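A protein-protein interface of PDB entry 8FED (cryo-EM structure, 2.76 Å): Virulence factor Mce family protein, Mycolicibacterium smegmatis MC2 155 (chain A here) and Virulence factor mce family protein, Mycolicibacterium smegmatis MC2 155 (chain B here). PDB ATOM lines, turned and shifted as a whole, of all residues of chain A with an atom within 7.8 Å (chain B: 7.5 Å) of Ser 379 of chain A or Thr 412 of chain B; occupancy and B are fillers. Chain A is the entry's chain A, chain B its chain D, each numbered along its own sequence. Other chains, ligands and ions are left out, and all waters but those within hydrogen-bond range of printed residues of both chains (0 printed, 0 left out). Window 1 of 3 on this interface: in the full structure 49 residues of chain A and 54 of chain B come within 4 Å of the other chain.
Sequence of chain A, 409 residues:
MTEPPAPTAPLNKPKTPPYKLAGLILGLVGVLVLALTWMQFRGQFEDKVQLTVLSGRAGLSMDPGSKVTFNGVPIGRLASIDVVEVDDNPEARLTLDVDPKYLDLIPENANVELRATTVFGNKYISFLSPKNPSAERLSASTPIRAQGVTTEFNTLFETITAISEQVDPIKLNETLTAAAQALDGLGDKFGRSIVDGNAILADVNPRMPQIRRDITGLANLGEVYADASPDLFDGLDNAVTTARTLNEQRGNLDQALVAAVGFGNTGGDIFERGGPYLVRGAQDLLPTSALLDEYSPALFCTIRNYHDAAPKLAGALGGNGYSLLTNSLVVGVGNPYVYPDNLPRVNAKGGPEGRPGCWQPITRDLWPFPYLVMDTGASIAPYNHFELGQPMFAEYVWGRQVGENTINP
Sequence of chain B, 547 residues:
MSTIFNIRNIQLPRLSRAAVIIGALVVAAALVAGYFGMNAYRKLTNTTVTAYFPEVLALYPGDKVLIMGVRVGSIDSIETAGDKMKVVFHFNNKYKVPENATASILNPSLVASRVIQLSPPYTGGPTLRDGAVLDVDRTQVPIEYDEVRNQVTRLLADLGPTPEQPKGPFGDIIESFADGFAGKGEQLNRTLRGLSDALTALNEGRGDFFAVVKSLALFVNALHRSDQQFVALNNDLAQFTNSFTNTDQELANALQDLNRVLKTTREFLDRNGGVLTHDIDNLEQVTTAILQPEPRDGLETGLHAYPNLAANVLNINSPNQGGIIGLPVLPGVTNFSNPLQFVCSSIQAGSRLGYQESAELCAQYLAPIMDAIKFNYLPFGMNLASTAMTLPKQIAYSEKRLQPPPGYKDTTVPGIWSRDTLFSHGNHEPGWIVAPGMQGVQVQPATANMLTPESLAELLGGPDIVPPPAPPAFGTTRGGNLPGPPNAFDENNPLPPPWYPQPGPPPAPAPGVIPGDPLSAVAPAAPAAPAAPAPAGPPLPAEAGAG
The backbone NH of Asn 335 of chain A is in hydrogen-bond range of the side-chain hydroxyl of Tyr 383 of chain A (3.0 Å). The backbone NH of Val 338 of chain A lies within hydrogen-bond range of the side-chain amide oxygen of Asn 342 of chain A (3.3 Å). The side-chain amide nitrogen (ND2) of Asn 342 of chain A sits at hydrogen-bond distance from the backbone carbonyl oxygen (O) of Gly 377 of chain A, 2.8 Å away. The backbone carbonyl oxygen of Met 374 of chain A sits close to the side-chain hydroxyl of Thr 376 of chain A (3.3 Å). The side-chain hydroxyl (OG1) of Thr 406 of chain A lies within hydrogen-bond range of the backbone NH (N) of Asn 408 of chain A. The backbone carbonyl oxygen (O) of Ile 416 of chain B lies close to the backbone NH (N) of Thr 411 of chain B (3.3 Å).
The backbone carbonyl oxygen of Ala 378 of chain A lies within hydrogen-bond range of the side-chain amide nitrogen of Asn 315 of chain B (3.3 Å). O of Thr 412 of chain B sits at hydrogen-bond distance from N of Ser 379 of chain A (2.7 Å). O of Ile 380 of chain A lies within hydrogen-bond range of OG1 of Thr 390 of chain B (3.5 Å). The backbone carbonyl oxygen (O) of Ala 381 of chain A is in hydrogen-bond range of the side-chain hydroxyl (OG1) of Thr 390 of chain B. O of Tyr 383 of chain A lies within hydrogen-bond range of N of Met 389 of chain B, 3.1 Å away. O of Tyr 383 of chain A sits at hydrogen-bond distance from N of Thr 390 of chain B (3.1 Å). The backbone carbonyl oxygen (O) of Ile 407 of chain A is in hydrogen-bond range of the backbone NH (N) of Thr 412 of chain B (2.8 Å). OH of Tyr 371 of chain A lies close to OD1 of Asn 315 of chain B, 2.3 Å away. OG of Ser 418 of chain B lies close to OD1 of Asn 408 of chain A, 2.4 Å away.
Among the printed residues, merely in contact across the chains: Ala 381 of chain A with Asp 410 of chain B, Pro 382 of chain A with Asp 410 of chain B, Asn 342 of chain A with Val 413 of chain B, Ala 378 of chain A with Thr 412 of chain B, Gly 377 of chain A with Val 413 of chain B, Met 374 of chain A with Pro 414 of chain B, Ile 407 of chain A with Thr 411 of chain B, Pro 382 of chain A with Thr 411 of chain B, Gly 377 of chain A with Pro 414 of chain B, Ala 378 of chain A with Pro 414 of chain B, Pro 382 of chain A with Thr 412 of chain B, Thr 376 of chain A with Ala 311 of chain B, Asp 341 of chain A with Val 413 of chain B, Ile 380 of chain A with Asn 315 of chain B, Ser 379 of chain A with Pro 414 of chain B, Pro 409 of chain A with Thr 412 of chain B, Ile 407 of chain A with Val 413 of chain B, Asn 408 of chain A with Thr 411 of chain B, Tyr 371 of chain A with Ile 395 of chain B, Asn 342 of chain A with Thr 412 of chain B, Tyr 383 of chain A with Thr 412 of chain B, Gly 377 of chain A with Thr 412 of chain B, Ser 379 of chain A with Asn 315 of chain B and Ile 380 of chain A with Met 389 of chain B.
Of the 22 printed residues of chain A, 15 touch a printed residue of chain B. Hydrophobic or aromatic side chains of chain A within 4 Å of the printed part of chain B: Tyr 371, Ala 378, Ile 380, Ala 381, Pro 382, Tyr 383, Ile 407 and Pro 409. Along chain A the printed residues that touch a printed residue of chain B span positions 341 to 409. Of the 13 printed residues of chain B, 11 touch a printed residue of chain A. Printed residues of chain B that touch a printed residue of chain A: Ala 311, Asn 315, Met 389, Thr 390, Ile 395, Asp 410, Thr 411, Thr 412, Val 413, Pro 414 and Ser 418. Among the printed residues, no Asp or Glu carboxylate lies within 4 Å of a Lys or Arg side-chain nitrogen of the other chain.
Val 338 of chain A touches none of the printed residues of chain B. Of the printed residues of chain B, Gly 377 of chain A touches Thr 412, Val 413 and Pro 414. Of chain B, only Asn 315 (3.9 Å), Thr 412 (2.7 Å) and Pro 414 (3.6 Å) come within 4 Å of Ser 379 of chain A. Printed residues of chain A within 4 Å of Asn 315 of chain B: Tyr 371, Ala 378, Ser 379 and Ile 380. Ile 416 of chain B touches none of the printed residues of chain A.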
ATOM      1  N   ASN A 335       7.226  -9.783 -21.851  1.00  0.00           N
ATOM      2  CA  ASN A 335       7.379  -9.775 -20.405  1.00  0.00           C
ATOM      3  C   ASN A 335       8.400  -8.719 -19.985  1.00  0.00           C
ATOM      4  O   ASN A 335       9.450  -8.583 -20.622  1.00  0.00           O
ATOM      5  CB  ASN A 335       7.822 -11.147 -19.906  1.00  0.00           C
ATOM      6  CG  ASN A 335       7.032 -12.275 -20.527  1.00  0.00           C
ATOM      7  OD1 ASN A 335       7.600 -13.224 -21.063  1.00  0.00           O
ATOM      8  ND2 ASN A 335       5.710 -12.175 -20.462  1.00  0.00           N
ATOM      9  N   PRO A 336       8.121  -7.959 -18.926  1.00  0.00           N
ATOM     10  CA  PRO A 336       9.119  -7.019 -18.407  1.00  0.00           C
ATOM     11  C   PRO A 336      10.383  -7.738 -17.959  1.00  0.00           C
ATOM     12  O   PRO A 336      10.399  -8.952 -17.740  1.00  0.00           O
ATOM     13  CB  PRO A 336       8.404  -6.361 -17.221  1.00  0.00           C
ATOM     14  CG  PRO A 336       6.958  -6.502 -17.533  1.00  0.00           C
ATOM     15  CD  PRO A 336       6.824  -7.818 -18.244  1.00  0.00           C
ATOM     16  N   TYR A 337      11.459  -6.969 -17.834  1.00  0.00           N
ATOM     17  CA  TYR A 337      12.741  -7.547 -17.463  1.00  0.00           C
ATOM     18  C   TYR A 337      12.724  -8.027 -16.017  1.00  0.00           C
ATOM     19  O   TYR A 337      12.141  -7.387 -15.138  1.00  0.00           O
ATOM     20  CB  TYR A 337      13.862  -6.530 -17.656  1.00  0.00           C
ATOM     21  CG  TYR A 337      13.955  -5.953 -19.049  1.00  0.00           C
ATOM     22  CD1 TYR A 337      14.504  -6.685 -20.090  1.00  0.00           C
ATOM     23  CD2 TYR A 337      13.529  -4.662 -19.313  1.00  0.00           C
ATOM     24  CE1 TYR A 337      14.597  -6.156 -21.361  1.00  0.00           C
ATOM     25  CE2 TYR A 337      13.627  -4.125 -20.578  1.00  0.00           C
ATOM     26  CZ  TYR A 337      14.156  -4.874 -21.598  1.00  0.00           C
ATOM     27  OH  TYR A 337      14.246  -4.332 -22.857  1.00  0.00           O
ATOM     28  N   VAL A 338      13.367  -9.167 -15.774  1.00  0.00           N
ATOM     29  CA  VAL A 338      13.539  -9.683 -14.421  1.00  0.00           C
ATOM     30  C   VAL A 338      14.713  -8.954 -13.781  1.00  0.00           C
ATOM     31  O   VAL A 338      15.499  -8.301 -14.476  1.00  0.00           O
ATOM     32  CB  VAL A 338      13.760 -11.206 -14.420  1.00  0.00           C
ATOM     33  CG1 VAL A 338      12.633 -11.901 -15.157  1.00  0.00           C
ATOM     34  CG2 VAL A 338      15.094 -11.543 -15.046  1.00  0.00           C
ATOM     35  N   ASP A 341      18.795 -11.290 -14.080  1.00  0.00           N
ATOM     36  CA  ASP A 341      19.282 -11.736 -15.383  1.00  0.00           C
ATOM     37  C   ASP A 341      19.385 -10.587 -16.377  1.00  0.00           C
ATOM     38  O   ASP A 341      20.363 -10.498 -17.128  1.00  0.00           O
ATOM     39  CB  ASP A 341      18.364 -12.824 -15.933  1.00  0.00           C
ATOM     40  CG  ASP A 341      18.282 -14.027 -15.027  1.00  0.00           C
ATOM     41  OD1 ASP A 341      19.344 -14.567 -14.668  1.00  0.00           O
ATOM     42  OD2 ASP A 341      17.156 -14.429 -14.669  1.00  0.00           O
ATOM     43  N   ASN A 342      18.390  -9.702 -16.405  1.00  0.00           N
ATOM     44  CA  ASN A 342      18.308  -8.654 -17.414  1.00  0.00           C
ATOM     45  C   ASN A 342      18.991  -7.362 -16.985  1.00  0.00           C
ATOM     46  O   ASN A 342      18.584  -6.278 -17.421  1.00  0.00           O
ATOM     47  CB  ASN A 342      16.846  -8.387 -17.773  1.00  0.00           C
ATOM     48  CG  ASN A 342      16.238  -9.491 -18.612  1.00  0.00           C
ATOM     49  OD1 ASN A 342      15.348 -10.210 -18.160  1.00  0.00           O
ATOM     50  ND2 ASN A 342      16.708  -9.627 -19.843  1.00  0.00           N
ATOM     51  N   TYR A 371      17.245  -8.902 -36.791  1.00  0.00           N
ATOM     52  CA  TYR A 371      17.481  -8.466 -35.424  1.00  0.00           C
ATOM     53  C   TYR A 371      18.888  -8.854 -34.994  1.00  0.00           C
ATOM     54  O   TYR A 371      19.313 -10.000 -35.171  1.00  0.00           O
ATOM     55  CB  TYR A 371      16.446  -9.067 -34.476  1.00  0.00           C
ATOM     56  CG  TYR A 371      16.464  -8.425 -33.109  1.00  0.00           C
ATOM     57  CD1 TYR A 371      15.802  -7.228 -32.878  1.00  0.00           C
ATOM     58  CD2 TYR A 371      17.154  -9.007 -32.056  1.00  0.00           C
ATOM     59  CE1 TYR A 371      15.823  -6.631 -31.636  1.00  0.00           C
ATOM     60  CE2 TYR A 371      17.180  -8.416 -30.810  1.00  0.00           C
ATOM     61  CZ  TYR A 371      16.514  -7.230 -30.607  1.00  0.00           C
ATOM     62  OH  TYR A 371      16.536  -6.642 -29.365  1.00  0.00           O
ATOM     63  N   LEU A 372      19.612  -7.893 -34.434  1.00  0.00           N
ATOM     64  CA  LEU A 372      21.003  -8.072 -34.038  1.00  0.00           C
ATOM     65  C   LEU A 372      21.065  -8.153 -32.520  1.00  0.00           C
ATOM     66  O   LEU A 372      20.864  -7.148 -31.830  1.00  0.00           O
ATOM     67  CB  LEU A 372      21.859  -6.924 -34.567  1.00  0.00           C
ATOM     68  CG  LEU A 372      23.372  -7.113 -34.537  1.00  0.00           C
ATOM     69  CD1 LEU A 372      23.780  -8.251 -35.451  1.00  0.00           C
ATOM     70  CD2 LEU A 372      24.062  -5.825 -34.939  1.00  0.00           C
ATOM     71  N   VAL A 373      21.337  -9.348 -32.004  1.00  0.00           N
ATOM     72  CA  VAL A 373      21.443  -9.573 -30.568  1.00  0.00           C
ATOM     73  C   VAL A 373      22.881  -9.323 -30.134  1.00  0.00           C
ATOM     74  O   VAL A 373      23.823  -9.903 -30.688  1.00  0.00           O
ATOM     75  CB  VAL A 373      20.980 -10.991 -30.192  1.00  0.00           C
ATOM     76  CG1 VAL A 373      19.473 -11.081 -30.263  1.00  0.00           C
ATOM     77  CG2 VAL A 373      21.588 -12.016 -31.120  1.00  0.00           C
ATOM     78  N   MET A 374      23.052  -8.451 -29.147  1.00  0.00           N
ATOM     79  CA  MET A 374      24.361  -8.048 -28.665  1.00  0.00           C
ATOM     80  C   MET A 374      24.469  -8.343 -27.176  1.00  0.00           C
ATOM     81  O   MET A 374      23.464  -8.459 -26.471  1.00  0.00           O
ATOM     82  CB  MET A 374      24.611  -6.562 -28.942  1.00  0.00           C
ATOM     83  CG  MET A 374      23.435  -5.668 -28.589  1.00  0.00           C
ATOM     84  SD  MET A 374      23.558  -4.024 -29.310  1.00  0.00           S
ATOM     85  CE  MET A 374      23.620  -4.434 -31.051  1.00  0.00           C
ATOM     86  N   THR A 376      24.301  -7.641 -24.112  1.00  0.00           N
ATOM     87  CA  THR A 376      23.756  -6.590 -23.269  1.00  0.00           C
ATOM     88  C   THR A 376      22.848  -7.116 -22.164  1.00  0.00           C
ATOM     89  O   THR A 376      22.484  -6.347 -21.268  1.00  0.00           O
ATOM     90  CB  THR A 376      22.982  -5.577 -24.127  1.00  0.00           C
ATOM     91  OG1 THR A 376      23.686  -5.371 -25.355  1.00  0.00           O
ATOM     92  CG2 THR A 376      22.873  -4.243 -23.427  1.00  0.00           C
ATOM     93  N   GLY A 377      22.491  -8.397 -22.180  1.00  0.00           N
ATOM     94  CA  GLY A 377      21.630  -8.959 -21.167  1.00  0.00           C
ATOM     95  C   GLY A 377      20.149  -8.805 -21.438  1.00  0.00           C
ATOM     96  O   GLY A 377      19.339  -9.377 -20.698  1.00  0.00           O
ATOM     97  N   ALA A 378      19.769  -8.058 -22.473  1.00  0.00           N
ATOM     98  CA  ALA A 378      18.377  -7.900 -22.863  1.00  0.00           C
ATOM     99  C   ALA A 378      18.233  -8.193 -24.348  1.00  0.00           C
ATOM    100  O   ALA A 378      19.078  -7.791 -25.153  1.00  0.00           O
ATOM    101  CB  ALA A 378      17.868  -6.493 -22.558  1.00  0.00           C
ATOM    102  N   SER A 379      17.160  -8.894 -24.704  1.00  0.00           N
ATOM    103  CA  SER A 379      16.928  -9.308 -26.080  1.00  0.00           C
ATOM    104  C   SER A 379      15.446  -9.605 -26.253  1.00  0.00           C
ATOM    105  O   SER A 379      14.698  -9.718 -25.281  1.00  0.00           O
ATOM    106  CB  SER A 379      17.778 -10.527 -26.449  1.00  0.00           C
ATOM    107  OG  SER A 379      17.350 -11.093 -27.673  1.00  0.00           O
ATOM    108  N   ILE A 380      15.027  -9.710 -27.514  1.00  0.00           N
ATOM    109  CA  ILE A 380      13.675 -10.151 -27.844  1.00  0.00           C
ATOM    110  C   ILE A 380      13.765 -11.283 -28.858  1.00  0.00           C
ATOM    111  O   ILE A 380      12.853 -11.488 -29.665  1.00  0.00           O
ATOM    112  CB  ILE A 380      12.806  -8.993 -28.366  1.00  0.00           C
ATOM    113  CG1 ILE A 380      13.413  -8.378 -29.625  1.00  0.00           C
ATOM    114  CG2 ILE A 380      12.617  -7.937 -27.290  1.00  0.00           C
ATOM    115  CD1 ILE A 380      12.605  -7.234 -30.179  1.00  0.00           C
ATOM    116  N   ALA A 381      14.869 -12.027 -28.811  1.00  0.00           N
ATOM    117  CA  ALA A 381      15.072 -13.146 -29.731  1.00  0.00           C
ATOM    118  C   ALA A 381      14.015 -14.243 -29.633  1.00  0.00           C
ATOM    119  O   ALA A 381      13.534 -14.690 -30.689  1.00  0.00           O
ATOM    120  CB  ALA A 381      16.475 -13.725 -29.526  1.00  0.00           C
ATOM    121  N   PRO A 382      13.608 -14.742 -28.436  1.00  0.00           N
ATOM    122  CA  PRO A 382      12.742 -15.930 -28.419  1.00  0.00           C
ATOM    123  C   PRO A 382      11.259 -15.613 -28.533  1.00  0.00           C
ATOM    124  O   PRO A 382      10.420 -16.465 -28.226  1.00  0.00           O
ATOM    125  CB  PRO A 382      13.062 -16.583 -27.068  1.00  0.00           C
ATOM    126  CG  PRO A 382      13.879 -15.583 -26.307  1.00  0.00           C
ATOM    127  CD  PRO A 382      13.876 -14.301 -27.059  1.00  0.00           C
ATOM    128  N   TYR A 383      10.920 -14.398 -28.962  1.00  0.00           N
ATOM    129  CA  TYR A 383       9.528 -14.028 -29.209  1.00  0.00           C
ATOM    130  C   TYR A 383       9.106 -14.467 -30.614  1.00  0.00           C
ATOM    131  O   TYR A 383       8.788 -13.663 -31.488  1.00  0.00           O
ATOM    132  CB  TYR A 383       9.335 -12.531 -29.017  1.00  0.00           C
ATOM    133  CG  TYR A 383       9.359 -12.084 -27.575  1.00  0.00           C
ATOM    134  CD1 TYR A 383       8.196 -12.056 -26.821  1.00  0.00           C
ATOM    135  CD2 TYR A 383      10.542 -11.681 -26.971  1.00  0.00           C
ATOM    136  CE1 TYR A 383       8.209 -11.645 -25.506  1.00  0.00           C
ATOM    137  CE2 TYR A 383      10.564 -11.266 -25.654  1.00  0.00           C
ATOM    138  CZ  TYR A 383       9.395 -11.250 -24.927  1.00  0.00           C
ATOM    139  OH  TYR A 383       9.411 -10.840 -23.616  1.00  0.00           O
ATOM    140  N   THR A 406      10.223 -15.056 -15.983  1.00  0.00           N
ATOM    141  CA  THR A 406      11.175 -15.906 -16.680  1.00  0.00           C
ATOM    142  C   THR A 406      11.849 -15.114 -17.786  1.00  0.00           C
ATOM    143  O   THR A 406      11.366 -14.063 -18.214  1.00  0.00           O
ATOM    144  CB  THR A 406      10.501 -17.152 -17.264  1.00  0.00           C
ATOM    145  OG1 THR A 406      11.478 -17.946 -17.946  1.00  0.00           O
ATOM    146  CG2 THR A 406       9.412 -16.755 -18.245  1.00  0.00           C
ATOM    147  N   ILE A 407      12.987 -15.636 -18.238  1.00  0.00           N
ATOM    148  CA  ILE A 407      13.709 -15.096 -19.380  1.00  0.00           C
ATOM    149  C   ILE A 407      13.589 -15.984 -20.603  1.00  0.00           C
ATOM    150  O   ILE A 407      14.224 -15.698 -21.629  1.00  0.00           O
ATOM    151  CB  ILE A 407      15.191 -14.853 -19.044  1.00  0.00           C
ATOM    152  CG1 ILE A 407      15.927 -16.183 -18.873  1.00  0.00           C
ATOM    153  CG2 ILE A 407      15.315 -14.011 -17.792  1.00  0.00           C
ATOM    154  CD1 ILE A 407      17.423 -16.038 -18.719  1.00  0.00           C
ATOM    155  N   ASN A 408      12.794 -17.048 -20.532  1.00  0.00           N
ATOM    156  CA  ASN A 408      12.642 -18.009 -21.624  1.00  0.00           C
ATOM    157  C   ASN A 408      11.155 -18.221 -21.895  1.00  0.00           C
ATOM    158  O   ASN A 408      10.578 -19.249 -21.522  1.00  0.00           O
ATOM    159  CB  ASN A 408      13.350 -19.322 -21.285  1.00  0.00           C
ATOM    160  CG  ASN A 408      13.087 -20.408 -22.297  1.00  0.00           C
ATOM    161  OD1 ASN A 408      13.746 -20.480 -23.331  1.00  0.00           O
ATOM    162  ND2 ASN A 408      12.117 -21.265 -22.005  1.00  0.00           N
ATOM    163  N   PRO A 409      10.487 -17.239 -22.521  1.00  0.00           N
ATOM    164  CA  PRO A 409       9.061 -17.410 -22.805  1.00  0.00           C
ATOM    165  C   PRO A 409       8.828 -18.273 -24.039  1.00  0.00           C
ATOM    166  O   PRO A 409       9.711 -18.413 -24.885  1.00  0.00           O
ATOM    167  CB  PRO A 409       8.580 -15.978 -23.036  1.00  0.00           C
ATOM    168  CG  PRO A 409       9.765 -15.284 -23.583  1.00  0.00           C
ATOM    169  CD  PRO A 409      10.969 -15.907 -22.932  1.00  0.00           C
ATOM    170  OXT PRO A 409       7.761 -18.859 -24.216  1.00  0.00           O
ATOM    171  N   ALA B 311      20.971   0.470 -26.472  1.00  0.00           N
ATOM    172  CA  ALA B 311      20.578  -0.933 -26.399  1.00  0.00           C
ATOM    173  C   ALA B 311      19.082  -1.078 -26.151  1.00  0.00           C
ATOM    174  O   ALA B 311      18.420  -1.928 -26.763  1.00  0.00           O
ATOM    175  CB  ALA B 311      21.371  -1.641 -25.309  1.00  0.00           C
ATOM    176  N   ASN B 315      16.212  -2.757 -28.531  1.00  0.00           N
ATOM    177  CA  ASN B 315      15.289  -3.799 -28.087  1.00  0.00           C
ATOM    178  C   ASN B 315      13.827  -3.374 -28.176  1.00  0.00           C
ATOM    179  O   ASN B 315      12.947  -4.238 -28.129  1.00  0.00           O
ATOM    180  CB  ASN B 315      15.619  -4.220 -26.657  1.00  0.00           C
ATOM    181  CG  ASN B 315      16.930  -4.966 -26.562  1.00  0.00           C
ATOM    182  OD1 ASN B 315      17.338  -5.647 -27.500  1.00  0.00           O
ATOM    183  ND2 ASN B 315      17.602  -4.838 -25.426  1.00  0.00           N
ATOM    184  N   MET B 389       7.322 -11.000 -31.828  1.00  0.00           N
ATOM    185  CA  MET B 389       8.056  -9.828 -32.295  1.00  0.00           C
ATOM    186  C   MET B 389       9.021 -10.180 -33.420  1.00  0.00           C
ATOM    187  O   MET B 389       9.112  -9.455 -34.415  1.00  0.00           O
ATOM    188  CB  MET B 389       8.805  -9.176 -31.135  1.00  0.00           C
ATOM    189  CG  MET B 389       7.909  -8.478 -30.128  1.00  0.00           C
ATOM    190  SD  MET B 389       8.847  -7.504 -28.937  1.00  0.00           S
ATOM    191  CE  MET B 389       7.522  -6.752 -27.999  1.00  0.00           C
ATOM    192  N   THR B 390       9.754 -11.277 -33.281  1.00  0.00           N
ATOM    193  CA  THR B 390      10.715 -11.710 -34.285  1.00  0.00           C
ATOM    194  C   THR B 390      10.361 -13.114 -34.766  1.00  0.00           C
ATOM    195  O   THR B 390       9.387 -13.723 -34.321  1.00  0.00           O
ATOM    196  CB  THR B 390      12.144 -11.677 -33.736  1.00  0.00           C
ATOM    197  OG1 THR B 390      12.345 -12.789 -32.857  1.00  0.00           O
ATOM    198  CG2 THR B 390      12.398 -10.388 -32.976  1.00  0.00           C
ATOM    199  N   ILE B 395      16.903 -13.642 -37.072  1.00  0.00           N
ATOM    200  CA  ILE B 395      17.821 -13.460 -35.953  1.00  0.00           C
ATOM    201  C   ILE B 395      19.250 -13.579 -36.465  1.00  0.00           C
ATOM    202  O   ILE B 395      19.661 -14.639 -36.949  1.00  0.00           O
ATOM    203  CB  ILE B 395      17.547 -14.476 -34.834  1.00  0.00           C
ATOM    204  CG1 ILE B 395      16.157 -14.243 -34.242  1.00  0.00           C
ATOM    205  CG2 ILE B 395      18.603 -14.369 -33.755  1.00  0.00           C
ATOM    206  CD1 ILE B 395      15.908 -12.815 -33.808  1.00  0.00           C
ATOM    207  N   ASP B 410      17.678 -19.607 -28.028  1.00  0.00           N
ATOM    208  CA  ASP B 410      18.112 -18.419 -27.310  1.00  0.00           C
ATOM    209  C   ASP B 410      17.048 -17.967 -26.316  1.00  0.00           C
ATOM    210  O   ASP B 410      15.855 -18.228 -26.489  1.00  0.00           O
ATOM    211  CB  ASP B 410      18.432 -17.288 -28.290  1.00  0.00           C
ATOM    212  CG  ASP B 410      19.251 -16.178 -27.657  1.00  0.00           C
ATOM    213  OD1 ASP B 410      20.367 -16.462 -27.175  1.00  0.00           O
ATOM    214  OD2 ASP B 410      18.788 -15.020 -27.650  1.00  0.00           O
ATOM    215  N   THR B 411      17.499 -17.293 -25.265  1.00  0.00           N
ATOM    216  CA  THR B 411      16.643 -16.701 -24.248  1.00  0.00           C
ATOM    217  C   THR B 411      16.681 -15.184 -24.373  1.00  0.00           C
ATOM    218  O   THR B 411      17.482 -14.622 -25.123  1.00  0.00           O
ATOM    219  CB  THR B 411      17.080 -17.130 -22.844  1.00  0.00           C
ATOM    220  OG1 THR B 411      18.437 -16.730 -22.625  1.00  0.00           O
ATOM    221  CG2 THR B 411      16.977 -18.631 -22.696  1.00  0.00           C
ATOM    222  N   THR B 412      15.800 -14.515 -23.626  1.00  0.00           N
ATOM    223  CA  THR B 412      15.734 -13.061 -23.704  1.00  0.00           C
ATOM    224  C   THR B 412      16.976 -12.386 -23.142  1.00  0.00           C
ATOM    225  O   THR B 412      17.135 -11.175 -23.323  1.00  0.00           O
ATOM    226  CB  THR B 412      14.499 -12.529 -22.977  1.00  0.00           C
ATOM    227  OG1 THR B 412      14.570 -12.877 -21.592  1.00  0.00           O
ATOM    228  CG2 THR B 412      13.238 -13.112 -23.580  1.00  0.00           C
ATOM    229  N   VAL B 413      17.842 -13.125 -22.455  1.00  0.00           N
ATOM    230  CA  VAL B 413      19.148 -12.629 -22.033  1.00  0.00           C
ATOM    231  C   VAL B 413      20.187 -13.238 -22.972  1.00  0.00           C
ATOM    232  O   VAL B 413      20.378 -14.464 -22.949  1.00  0.00           O
ATOM    233  CB  VAL B 413      19.444 -12.986 -20.572  1.00  0.00           C
ATOM    234  CG1 VAL B 413      20.761 -12.378 -20.133  1.00  0.00           C
ATOM    235  CG2 VAL B 413      18.318 -12.512 -19.679  1.00  0.00           C
ATOM    236  N   PRO B 414      20.843 -12.446 -23.821  1.00  0.00           N
ATOM    237  CA  PRO B 414      21.828 -13.014 -24.752  1.00  0.00           C
ATOM    238  C   PRO B 414      22.957 -13.718 -24.017  1.00  0.00           C
ATOM    239  O   PRO B 414      23.436 -13.253 -22.982  1.00  0.00           O
ATOM    240  CB  PRO B 414      22.338 -11.788 -25.518  1.00  0.00           C
ATOM    241  CG  PRO B 414      21.256 -10.774 -25.376  1.00  0.00           C
ATOM    242  CD  PRO B 414      20.651 -11.004 -24.030  1.00  0.00           C
ATOM    243  N   GLY B 415      23.383 -14.848 -24.568  1.00  0.00           N
ATOM    244  CA  GLY B 415      24.412 -15.660 -23.971  1.00  0.00           C
ATOM    245  C   GLY B 415      23.901 -16.808 -23.127  1.00  0.00           C
ATOM    246  O   GLY B 415      24.660 -17.745 -22.862  1.00  0.00           O
ATOM    247  N   ILE B 416      22.642 -16.764 -22.698  1.00  0.00           N
ATOM    248  CA  ILE B 416      22.027 -17.852 -21.947  1.00  0.00           C
ATOM    249  C   ILE B 416      21.116 -18.623 -22.891  1.00  0.00           C
ATOM    250  O   ILE B 416      20.134 -18.078 -23.407  1.00  0.00           O
ATOM    251  CB  ILE B 416      21.245 -17.325 -20.734  1.00  0.00           C
ATOM    252  CG1 ILE B 416      22.155 -16.490 -19.833  1.00  0.00           C
ATOM    253  CG2 ILE B 416      20.642 -18.480 -19.958  1.00  0.00           C
ATOM    254  CD1 ILE B 416      21.458 -15.938 -18.614  1.00  0.00           C
ATOM    255  N   SER B 418      18.629 -21.779 -23.639  1.00  0.00           N
ATOM    256  CA  SER B 418      17.753 -22.793 -23.077  1.00  0.00           C
ATOM    257  C   SER B 418      17.583 -23.946 -24.061  1.00  0.00           C
ATOM    258  O   SER B 418      18.145 -23.949 -25.156  1.00  0.00           O
ATOM    259  CB  SER B 418      16.402 -22.190 -22.704  1.00  0.00           C
ATOM    260  OG  SER B 418      15.819 -21.529 -23.809  1.00  0.00           O
